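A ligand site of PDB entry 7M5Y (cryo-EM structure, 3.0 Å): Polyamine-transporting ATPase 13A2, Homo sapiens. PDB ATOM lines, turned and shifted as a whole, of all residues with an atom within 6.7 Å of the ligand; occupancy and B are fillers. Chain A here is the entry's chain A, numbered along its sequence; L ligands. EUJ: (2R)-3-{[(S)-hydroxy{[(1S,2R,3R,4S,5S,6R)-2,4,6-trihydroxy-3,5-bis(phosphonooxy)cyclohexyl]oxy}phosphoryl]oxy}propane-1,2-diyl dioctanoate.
The side-chain hydroxyl of Ser 1155 lies within hydrogen-bond range of an oxygen (O33) of the ligand (2.9 Å). The backbone NH (N) of Gly 994 lies close to an oxygen (O53) of the ligand (3.2 Å). The backbone NH (N) of Ala 995 is in hydrogen-bond range of an oxygen (O53) of the ligand (3.0 Å).
The side-chain hydroxyl (OG) of Ser 998 sits close to the backbone carbonyl oxygen (O) of Ala 995, at 3.3 Å.
Val 999 touches the ligand. Leu 1146 touches the ligand. Arg 1147 touches the ligand. Six residues have an atom within 4 Å of the ligand: Gly 994, Ala 995, Val 999, Leu 1146, Arg 1147 and Ser 1155. Along chain A the residues within 4 Å of the ligand span positions 994 to 1155. The nearest printed residue that does not touch the ligand is Ser 998 (4.2 Å).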
ATOM      1  N   PHE A 931      32.424  35.406 -31.292  1.00  0.00           N
ATOM      2  CA  PHE A 931      31.842  34.077 -31.306  1.00  0.00           C
ATOM      3  C   PHE A 931      31.558  33.611 -32.729  1.00  0.00           C
ATOM      4  O   PHE A 931      32.112  32.589 -33.180  1.00  0.00           O
ATOM      5  CB  PHE A 931      30.548  34.066 -30.490  1.00  0.00           C
ATOM      6  CG  PHE A 931      30.718  33.593 -29.074  1.00  0.00           C
ATOM      7  CD1 PHE A 931      31.655  34.194 -28.238  1.00  0.00           C
ATOM      8  CD2 PHE A 931      29.952  32.560 -28.583  1.00  0.00           C
ATOM      9  CE1 PHE A 931      31.812  33.763 -26.938  1.00  0.00           C
ATOM     10  CE2 PHE A 931      30.109  32.128 -27.282  1.00  0.00           C
ATOM     11  CZ  PHE A 931      31.036  32.727 -26.457  1.00  0.00           C
ATOM     12  N   PRO A 992      25.558  38.500 -23.522  1.00  0.00           N
ATOM     13  CA  PRO A 992      25.910  37.466 -24.503  1.00  0.00           C
ATOM     14  C   PRO A 992      26.523  36.267 -23.812  1.00  0.00           C
ATOM     15  O   PRO A 992      26.866  36.337 -22.622  1.00  0.00           O
ATOM     16  CB  PRO A 992      26.918  38.174 -25.410  1.00  0.00           C
ATOM     17  CG  PRO A 992      27.533  39.194 -24.551  1.00  0.00           C
ATOM     18  CD  PRO A 992      26.467  39.659 -23.620  1.00  0.00           C
ATOM     19  N   PRO A 993      26.666  35.129 -24.506  1.00  0.00           N
ATOM     20  CA  PRO A 993      27.343  33.990 -23.882  1.00  0.00           C
ATOM     21  C   PRO A 993      28.775  34.324 -23.502  1.00  0.00           C
ATOM     22  O   PRO A 993      29.489  35.015 -24.239  1.00  0.00           O
ATOM     23  CB  PRO A 993      27.288  32.911 -24.975  1.00  0.00           C
ATOM     24  CG  PRO A 993      26.181  33.311 -25.871  1.00  0.00           C
ATOM     25  CD  PRO A 993      26.170  34.813 -25.854  1.00  0.00           C
ATOM     26  N   GLY A 994      29.188  33.833 -22.339  1.00  0.00           N
ATOM     27  CA  GLY A 994      30.505  34.130 -21.800  1.00  0.00           C
ATOM     28  C   GLY A 994      31.541  33.055 -22.039  1.00  0.00           C
ATOM     29  O   GLY A 994      32.633  33.108 -21.447  1.00  0.00           O
ATOM     30  N   ALA A 995      31.248  32.074 -22.891  1.00  0.00           N
ATOM     31  CA  ALA A 995      32.149  30.941 -23.077  1.00  0.00           C
ATOM     32  C   ALA A 995      31.935  30.231 -24.404  1.00  0.00           C
ATOM     33  O   ALA A 995      30.816  29.817 -24.722  1.00  0.00           O
ATOM     34  CB  ALA A 995      31.974  29.942 -21.930  1.00  0.00           C
ATOM     35  N   LEU A 996      33.009  30.095 -25.184  1.00  0.00           N
ATOM     36  CA  LEU A 996      32.945  29.399 -26.462  1.00  0.00           C
ATOM     37  C   LEU A 996      32.705  27.903 -26.314  1.00  0.00           C
ATOM     38  O   LEU A 996      32.200  27.282 -27.258  1.00  0.00           O
ATOM     39  CB  LEU A 996      34.233  29.613 -27.256  1.00  0.00           C
ATOM     40  CG  LEU A 996      34.415  30.938 -28.011  1.00  0.00           C
ATOM     41  CD1 LEU A 996      35.768  30.944 -28.673  1.00  0.00           C
ATOM     42  CD2 LEU A 996      33.329  31.142 -29.044  1.00  0.00           C
ATOM     43  N   LEU A 997      33.040  27.319 -25.166  1.00  0.00           N
ATOM     44  CA  LEU A 997      32.791  25.896 -24.944  1.00  0.00           C
ATOM     45  C   LEU A 997      31.400  25.623 -24.387  1.00  0.00           C
ATOM     46  O   LEU A 997      31.177  24.566 -23.790  1.00  0.00           O
ATOM     47  CB  LEU A 997      33.857  25.329 -23.993  1.00  0.00           C
ATOM     48  CG  LEU A 997      34.079  25.934 -22.600  1.00  0.00           C
ATOM     49  CD1 LEU A 997      32.994  25.550 -21.587  1.00  0.00           C
ATOM     50  CD2 LEU A 997      35.455  25.551 -22.061  1.00  0.00           C
ATOM     51  N   SER A 998      30.459  26.541 -24.586  1.00  0.00           N
ATOM     52  CA  SER A 998      29.114  26.381 -24.058  1.00  0.00           C
ATOM     53  C   SER A 998      28.382  25.275 -24.824  1.00  0.00           C
ATOM     54  O   SER A 998      28.775  24.884 -25.924  1.00  0.00           O
ATOM     55  CB  SER A 998      28.349  27.697 -24.135  1.00  0.00           C
ATOM     56  OG  SER A 998      28.113  28.070 -25.485  1.00  0.00           O
ATOM     57  N   VAL A 999      27.324  24.759 -24.199  1.00  0.00           N
ATOM     58  CA  VAL A 999      26.503  23.742 -24.857  1.00  0.00           C
ATOM     59  C   VAL A 999      25.954  24.228 -26.187  1.00  0.00           C
ATOM     60  O   VAL A 999      26.033  23.473 -27.172  1.00  0.00           O
ATOM     61  CB  VAL A 999      25.397  23.271 -23.895  1.00  0.00           C
ATOM     62  CG1 VAL A 999      24.387  22.389 -24.619  1.00  0.00           C
ATOM     63  CG2 VAL A 999      26.007  22.530 -22.711  1.00  0.00           C
ATOM     64  N   PRO A1000      25.358  25.430 -26.304  1.00  0.00           N
ATOM     65  CA  PRO A1000      24.869  25.861 -27.621  1.00  0.00           C
ATOM     66  C   PRO A1000      25.929  25.919 -28.709  1.00  0.00           C
ATOM     67  O   PRO A1000      25.677  25.482 -29.828  1.00  0.00           O
ATOM     68  CB  PRO A1000      24.265  27.249 -27.340  1.00  0.00           C
ATOM     69  CG  PRO A1000      24.715  27.619 -25.979  1.00  0.00           C
ATOM     70  CD  PRO A1000      24.876  26.345 -25.251  1.00  0.00           C
ATOM     71  N   LEU A1002      28.872  24.247 -28.962  1.00  0.00           N
ATOM     72  CA  LEU A1002      29.331  22.908 -29.331  1.00  0.00           C
ATOM     73  C   LEU A1002      28.246  22.166 -30.111  1.00  0.00           C
ATOM     74  O   LEU A1002      28.546  21.507 -31.122  1.00  0.00           O
ATOM     75  CB  LEU A1002      29.713  22.135 -28.067  1.00  0.00           C
ATOM     76  CG  LEU A1002      30.289  20.722 -28.224  1.00  0.00           C
ATOM     77  CD1 LEU A1002      31.599  20.763 -29.003  1.00  0.00           C
ATOM     78  CD2 LEU A1002      30.487  20.080 -26.858  1.00  0.00           C
ATOM     79  N   PRO A1143      17.261  26.796 -25.461  1.00  0.00           N
ATOM     80  CA  PRO A1143      17.134  27.161 -24.045  1.00  0.00           C
ATOM     81  C   PRO A1143      15.944  26.519 -23.354  1.00  0.00           C
ATOM     82  O   PRO A1143      16.056  26.133 -22.180  1.00  0.00           O
ATOM     83  CB  PRO A1143      17.008  28.685 -24.082  1.00  0.00           C
ATOM     84  CG  PRO A1143      17.674  29.092 -25.320  1.00  0.00           C
ATOM     85  CD  PRO A1143      17.427  27.999 -26.303  1.00  0.00           C
ATOM     86  N   CYS A1145      14.535  23.566 -24.031  1.00  0.00           N
ATOM     87  CA  CYS A1145      14.842  22.177 -23.740  1.00  0.00           C
ATOM     88  C   CYS A1145      15.852  22.054 -22.609  1.00  0.00           C
ATOM     89  O   CYS A1145      15.730  21.166 -21.758  1.00  0.00           O
ATOM     90  CB  CYS A1145      15.365  21.488 -25.002  1.00  0.00           C
ATOM     91  SG  CYS A1145      14.268  21.634 -26.433  1.00  0.00           S
ATOM     92  N   LEU A1146      16.868  22.919 -22.599  1.00  0.00           N
ATOM     93  CA  LEU A1146      17.864  22.872 -21.531  1.00  0.00           C
ATOM     94  C   LEU A1146      17.234  23.160 -20.168  1.00  0.00           C
ATOM     95  O   LEU A1146      17.535  22.473 -19.183  1.00  0.00           O
ATOM     96  CB  LEU A1146      18.982  23.858 -21.827  1.00  0.00           C
ATOM     97  CG  LEU A1146      19.866  23.535 -23.040  1.00  0.00           C
ATOM     98  CD1 LEU A1146      20.815  24.693 -23.328  1.00  0.00           C
ATOM     99  CD2 LEU A1146      20.657  22.243 -22.833  1.00  0.00           C
ATOM    100  N   ARG A1147      16.383  24.179 -20.096  1.00  0.00           N
ATOM    101  CA  ARG A1147      15.722  24.529 -18.836  1.00  0.00           C
ATOM    102  C   ARG A1147      14.731  23.462 -18.398  1.00  0.00           C
ATOM    103  O   ARG A1147      14.654  23.145 -17.203  1.00  0.00           O
ATOM    104  CB  ARG A1147      15.032  25.890 -18.966  1.00  0.00           C
ATOM    105  CG  ARG A1147      15.968  27.090 -19.190  1.00  0.00           C
ATOM    106  CD  ARG A1147      16.748  27.554 -17.942  1.00  0.00           C
ATOM    107  NE  ARG A1147      17.734  26.589 -17.466  1.00  0.00           N
ATOM    108  CZ  ARG A1147      18.866  26.274 -18.084  1.00  0.00           C
ATOM    109  NH1 ARG A1147      19.216  26.854 -19.231  1.00  0.00           N
ATOM    110  NH2 ARG A1147      19.671  25.356 -17.551  1.00  0.00           N
ATOM    111  N   LEU A1149      14.923  20.420 -18.718  1.00  0.00           N
ATOM    112  CA  LEU A1149      15.634  19.253 -18.221  1.00  0.00           C
ATOM    113  C   LEU A1149      16.569  19.711 -17.113  1.00  0.00           C
ATOM    114  O   LEU A1149      17.432  20.573 -17.342  1.00  0.00           O
ATOM    115  CB  LEU A1149      16.406  18.582 -19.360  1.00  0.00           C
ATOM    116  CG  LEU A1149      17.085  17.211 -19.157  1.00  0.00           C
ATOM    117  CD1 LEU A1149      17.575  16.693 -20.504  1.00  0.00           C
ATOM    118  CD2 LEU A1149      18.245  17.236 -18.165  1.00  0.00           C
ATOM    119  N   ARG A1150      16.426  19.127 -15.926  1.00  0.00           N
ATOM    120  CA  ARG A1150      17.265  19.495 -14.785  1.00  0.00           C
ATOM    121  C   ARG A1150      17.098  20.976 -14.452  1.00  0.00           C
ATOM    122  O   ARG A1150      18.052  21.756 -14.572  1.00  0.00           O
ATOM    123  CB  ARG A1150      18.735  19.183 -15.063  1.00  0.00           C
ATOM    124  N   ARG A1153      19.394  24.613 -11.629  1.00  0.00           N
ATOM    125  CA  ARG A1153      20.621  25.140 -12.221  1.00  0.00           C
ATOM    126  C   ARG A1153      21.692  25.421 -11.168  1.00  0.00           C
ATOM    127  O   ARG A1153      22.751  24.781 -11.164  1.00  0.00           O
ATOM    128  CB  ARG A1153      20.322  26.417 -13.005  1.00  0.00           C
ATOM    129  N   ALA A1154      21.395  26.363 -10.281  1.00  0.00           N
ATOM    130  CA  ALA A1154      22.246  26.758  -9.156  1.00  0.00           C
ATOM    131  C   ALA A1154      23.667  27.120  -9.623  1.00  0.00           C
ATOM    132  O   ALA A1154      24.649  26.442  -9.336  1.00  0.00           O
ATOM    133  CB  ALA A1154      22.295  25.660  -8.097  1.00  0.00           C
ATOM    134  N   SER A1155      23.697  28.216 -10.389  1.00  0.00           N
ATOM    135  CA  SER A1155      24.874  28.708 -11.095  1.00  0.00           C
ATOM    136  C   SER A1155      26.107  28.805 -10.200  1.00  0.00           C
ATOM    137  O   SER A1155      26.040  29.216  -9.044  1.00  0.00           O
ATOM    138  CB  SER A1155      24.583  30.071 -11.706  1.00  0.00           C
ATOM    139  OG  SER A1155      25.530  30.401 -12.712  1.00  0.00           O
ATOM    140  N   LYS A1156      27.266  28.414 -10.758  1.00  0.00           N
ATOM    141  CA  LYS A1156      28.485  28.211  -9.985  1.00  0.00           C
ATOM    142  C   LYS A1156      29.233  29.502  -9.674  1.00  0.00           C
ATOM    143  O   LYS A1156      30.159  29.475  -8.863  1.00  0.00           O
ATOM    144  CB  LYS A1156      29.451  27.275 -10.726  1.00  0.00           C
ATOM    145  CG  LYS A1156      28.928  25.893 -11.117  1.00  0.00           C
ATOM    146  CD  LYS A1156      28.650  25.034  -9.869  1.00  0.00           C
ATOM    147  CE  LYS A1156      27.223  25.068  -9.363  1.00  0.00           C
ATOM    148  NZ  LYS A1156      27.037  24.118  -8.235  1.00  0.00           N
ATOM    149  N   LYS A1157      28.870  30.627 -10.293  1.00  0.00           N
ATOM    150  CA  LYS A1157      29.579  31.867 -10.023  1.00  0.00           C
ATOM    151  C   LYS A1157      29.388  32.271  -8.573  1.00  0.00           C
ATOM    152  O   LYS A1157      28.291  32.164  -8.018  1.00  0.00           O
ATOM    153  CB  LYS A1157      29.086  32.975 -10.961  1.00  0.00           C
ATOM    154  CG  LYS A1157      29.219  32.615 -12.444  1.00  0.00           C
ATOM    155  CD  LYS A1157      28.880  33.785 -13.356  1.00  0.00           C
ATOM    156  CE  LYS A1157      30.082  34.677 -13.602  1.00  0.00           C
ATOM    157  NZ  LYS A1157      31.099  34.026 -14.485  1.00  0.00           N
ATOM    158  N   LYS A1160      26.701  35.040  -7.657  1.00  0.00           N
ATOM    159  CA  LYS A1160      25.323  34.579  -7.781  1.00  0.00           C
ATOM    160  C   LYS A1160      24.932  33.699  -6.599  1.00  0.00           C
ATOM    161  O   LYS A1160      23.826  33.815  -6.043  1.00  0.00           O
ATOM    162  CB  LYS A1160      25.141  33.815  -9.089  1.00  0.00           C
ATOM    163  CG  LYS A1160      25.406  34.616 -10.361  1.00  0.00           C
ATOM    164  CD  LYS A1160      24.265  35.569 -10.692  1.00  0.00           C
ATOM    165  CE  LYS A1160      23.068  34.838 -11.305  1.00  0.00           C
ATOM    166  NZ  LYS A1160      21.951  35.758 -11.624  1.00  0.00           N
HETATM  167  C1  EUJ L   1      26.940  27.288 -17.838  1.00  0.00           C
HETATM  168  C2  EUJ L   1      25.785  28.035 -17.171  1.00  0.00           C
HETATM  169  C3  EUJ L   1      26.215  29.339 -16.523  1.00  0.00           C
HETATM  170  C4  EUJ L   1      27.342  30.079 -17.184  1.00  0.00           C
HETATM  171  C5  EUJ L   1      28.577  29.221 -17.395  1.00  0.00           C
HETATM  172  C6  EUJ L   1      28.308  27.720 -17.338  1.00  0.00           C
HETATM  173  O1  EUJ L   1      26.798  27.443 -19.294  1.00  0.00           O
HETATM  174  O2  EUJ L   1      24.781  28.329 -18.144  1.00  0.00           O
HETATM  175  O3  EUJ L   1      25.130  30.289 -16.689  1.00  0.00           O
HETATM  176  O4  EUJ L   1      26.891  30.570 -18.440  1.00  0.00           O
HETATM  177  O5  EUJ L   1      29.126  29.543 -18.721  1.00  0.00           O
HETATM  178  O6  EUJ L   1      28.449  27.298 -15.984  1.00  0.00           O
HETATM  179  P1  EUJ L   1      25.807  26.467 -20.055  1.00  0.00           P
HETATM  180  O11 EUJ L   1      26.605  25.426 -20.790  1.00  0.00           O
HETATM  181  O12 EUJ L   1      24.806  27.283 -20.844  1.00  0.00           O
HETATM  182  O13 EUJ L   1      25.045  25.761 -18.828  1.00  0.00           O
HETATM  183  P3  EUJ L   1      23.813  30.352 -15.826  1.00  0.00           P
HETATM  184  O31 EUJ L   1      23.813  31.701 -15.127  1.00  0.00           O
HETATM  185  O32 EUJ L   1      22.650  30.202 -16.788  1.00  0.00           O
HETATM  186  O33 EUJ L   1      23.895  29.201 -14.837  1.00  0.00           O
HETATM  187  P5  EUJ L   1      29.954  30.903 -18.953  1.00  0.00           P
HETATM  188  O51 EUJ L   1      31.413  30.561 -18.705  1.00  0.00           O
HETATM  189  O52 EUJ L   1      29.437  31.924 -17.959  1.00  0.00           O
HETATM  190  O53 EUJ L   1      29.707  31.325 -20.383  1.00  0.00           O
HETATM  191  C1A EUJ L   1      22.128  22.393 -19.152  1.00  0.00           C
HETATM  192  C1B EUJ L   1      27.186  22.505 -19.256  1.00  0.00           C
HETATM  193  C1C EUJ L   1      23.885  24.913 -19.042  1.00  0.00           C
HETATM  194  C2A EUJ L   1      21.841  20.954 -19.381  1.00  0.00           C
HETATM  195  C2B EUJ L   1      28.604  22.347 -18.837  1.00  0.00           C
HETATM  196  C2C EUJ L   1      24.253  23.419 -18.789  1.00  0.00           C
HETATM  197  C3A EUJ L   1      22.788  20.323 -20.340  1.00  0.00           C
HETATM  198  C3B EUJ L   1      29.527  22.224 -19.992  1.00  0.00           C
HETATM  199  C3C EUJ L   1      25.459  23.291 -17.898  1.00  0.00           C
HETATM  200  C4A EUJ L   1      22.984  18.820 -20.017  1.00  0.00           C
HETATM  201  C4B EUJ L   1      29.573  20.813 -20.562  1.00  0.00           C
HETATM  202  C5A EUJ L   1      23.884  18.143 -21.019  1.00  0.00           C
HETATM  203  C5B EUJ L   1      29.844  20.759 -22.036  1.00  0.00           C
HETATM  204  C6A EUJ L   1      25.100  17.534 -20.405  1.00  0.00           C
HETATM  205  C6B EUJ L   1      29.728  19.382 -22.645  1.00  0.00           C
HETATM  206  C7A EUJ L   1      26.388  17.748 -21.170  1.00  0.00           C
HETATM  207  C7B EUJ L   1      30.738  18.385 -22.156  1.00  0.00           C
HETATM  208  C8A EUJ L   1      27.470  16.724 -20.865  1.00  0.00           C
HETATM  209  C8B EUJ L   1      30.884  17.204 -23.074  1.00  0.00           C
HETATM  210  O1A EUJ L   1      21.528  23.282 -19.708  1.00  0.00           O
HETATM  211  O1B EUJ L   1      26.588  21.741 -19.977  1.00  0.00           O
HETATM  212  O2C EUJ L   1      23.104  22.685 -18.278  1.00  0.00           O
HETATM  213  O3C EUJ L   1      26.621  23.576 -18.705  1.00  0.00           O
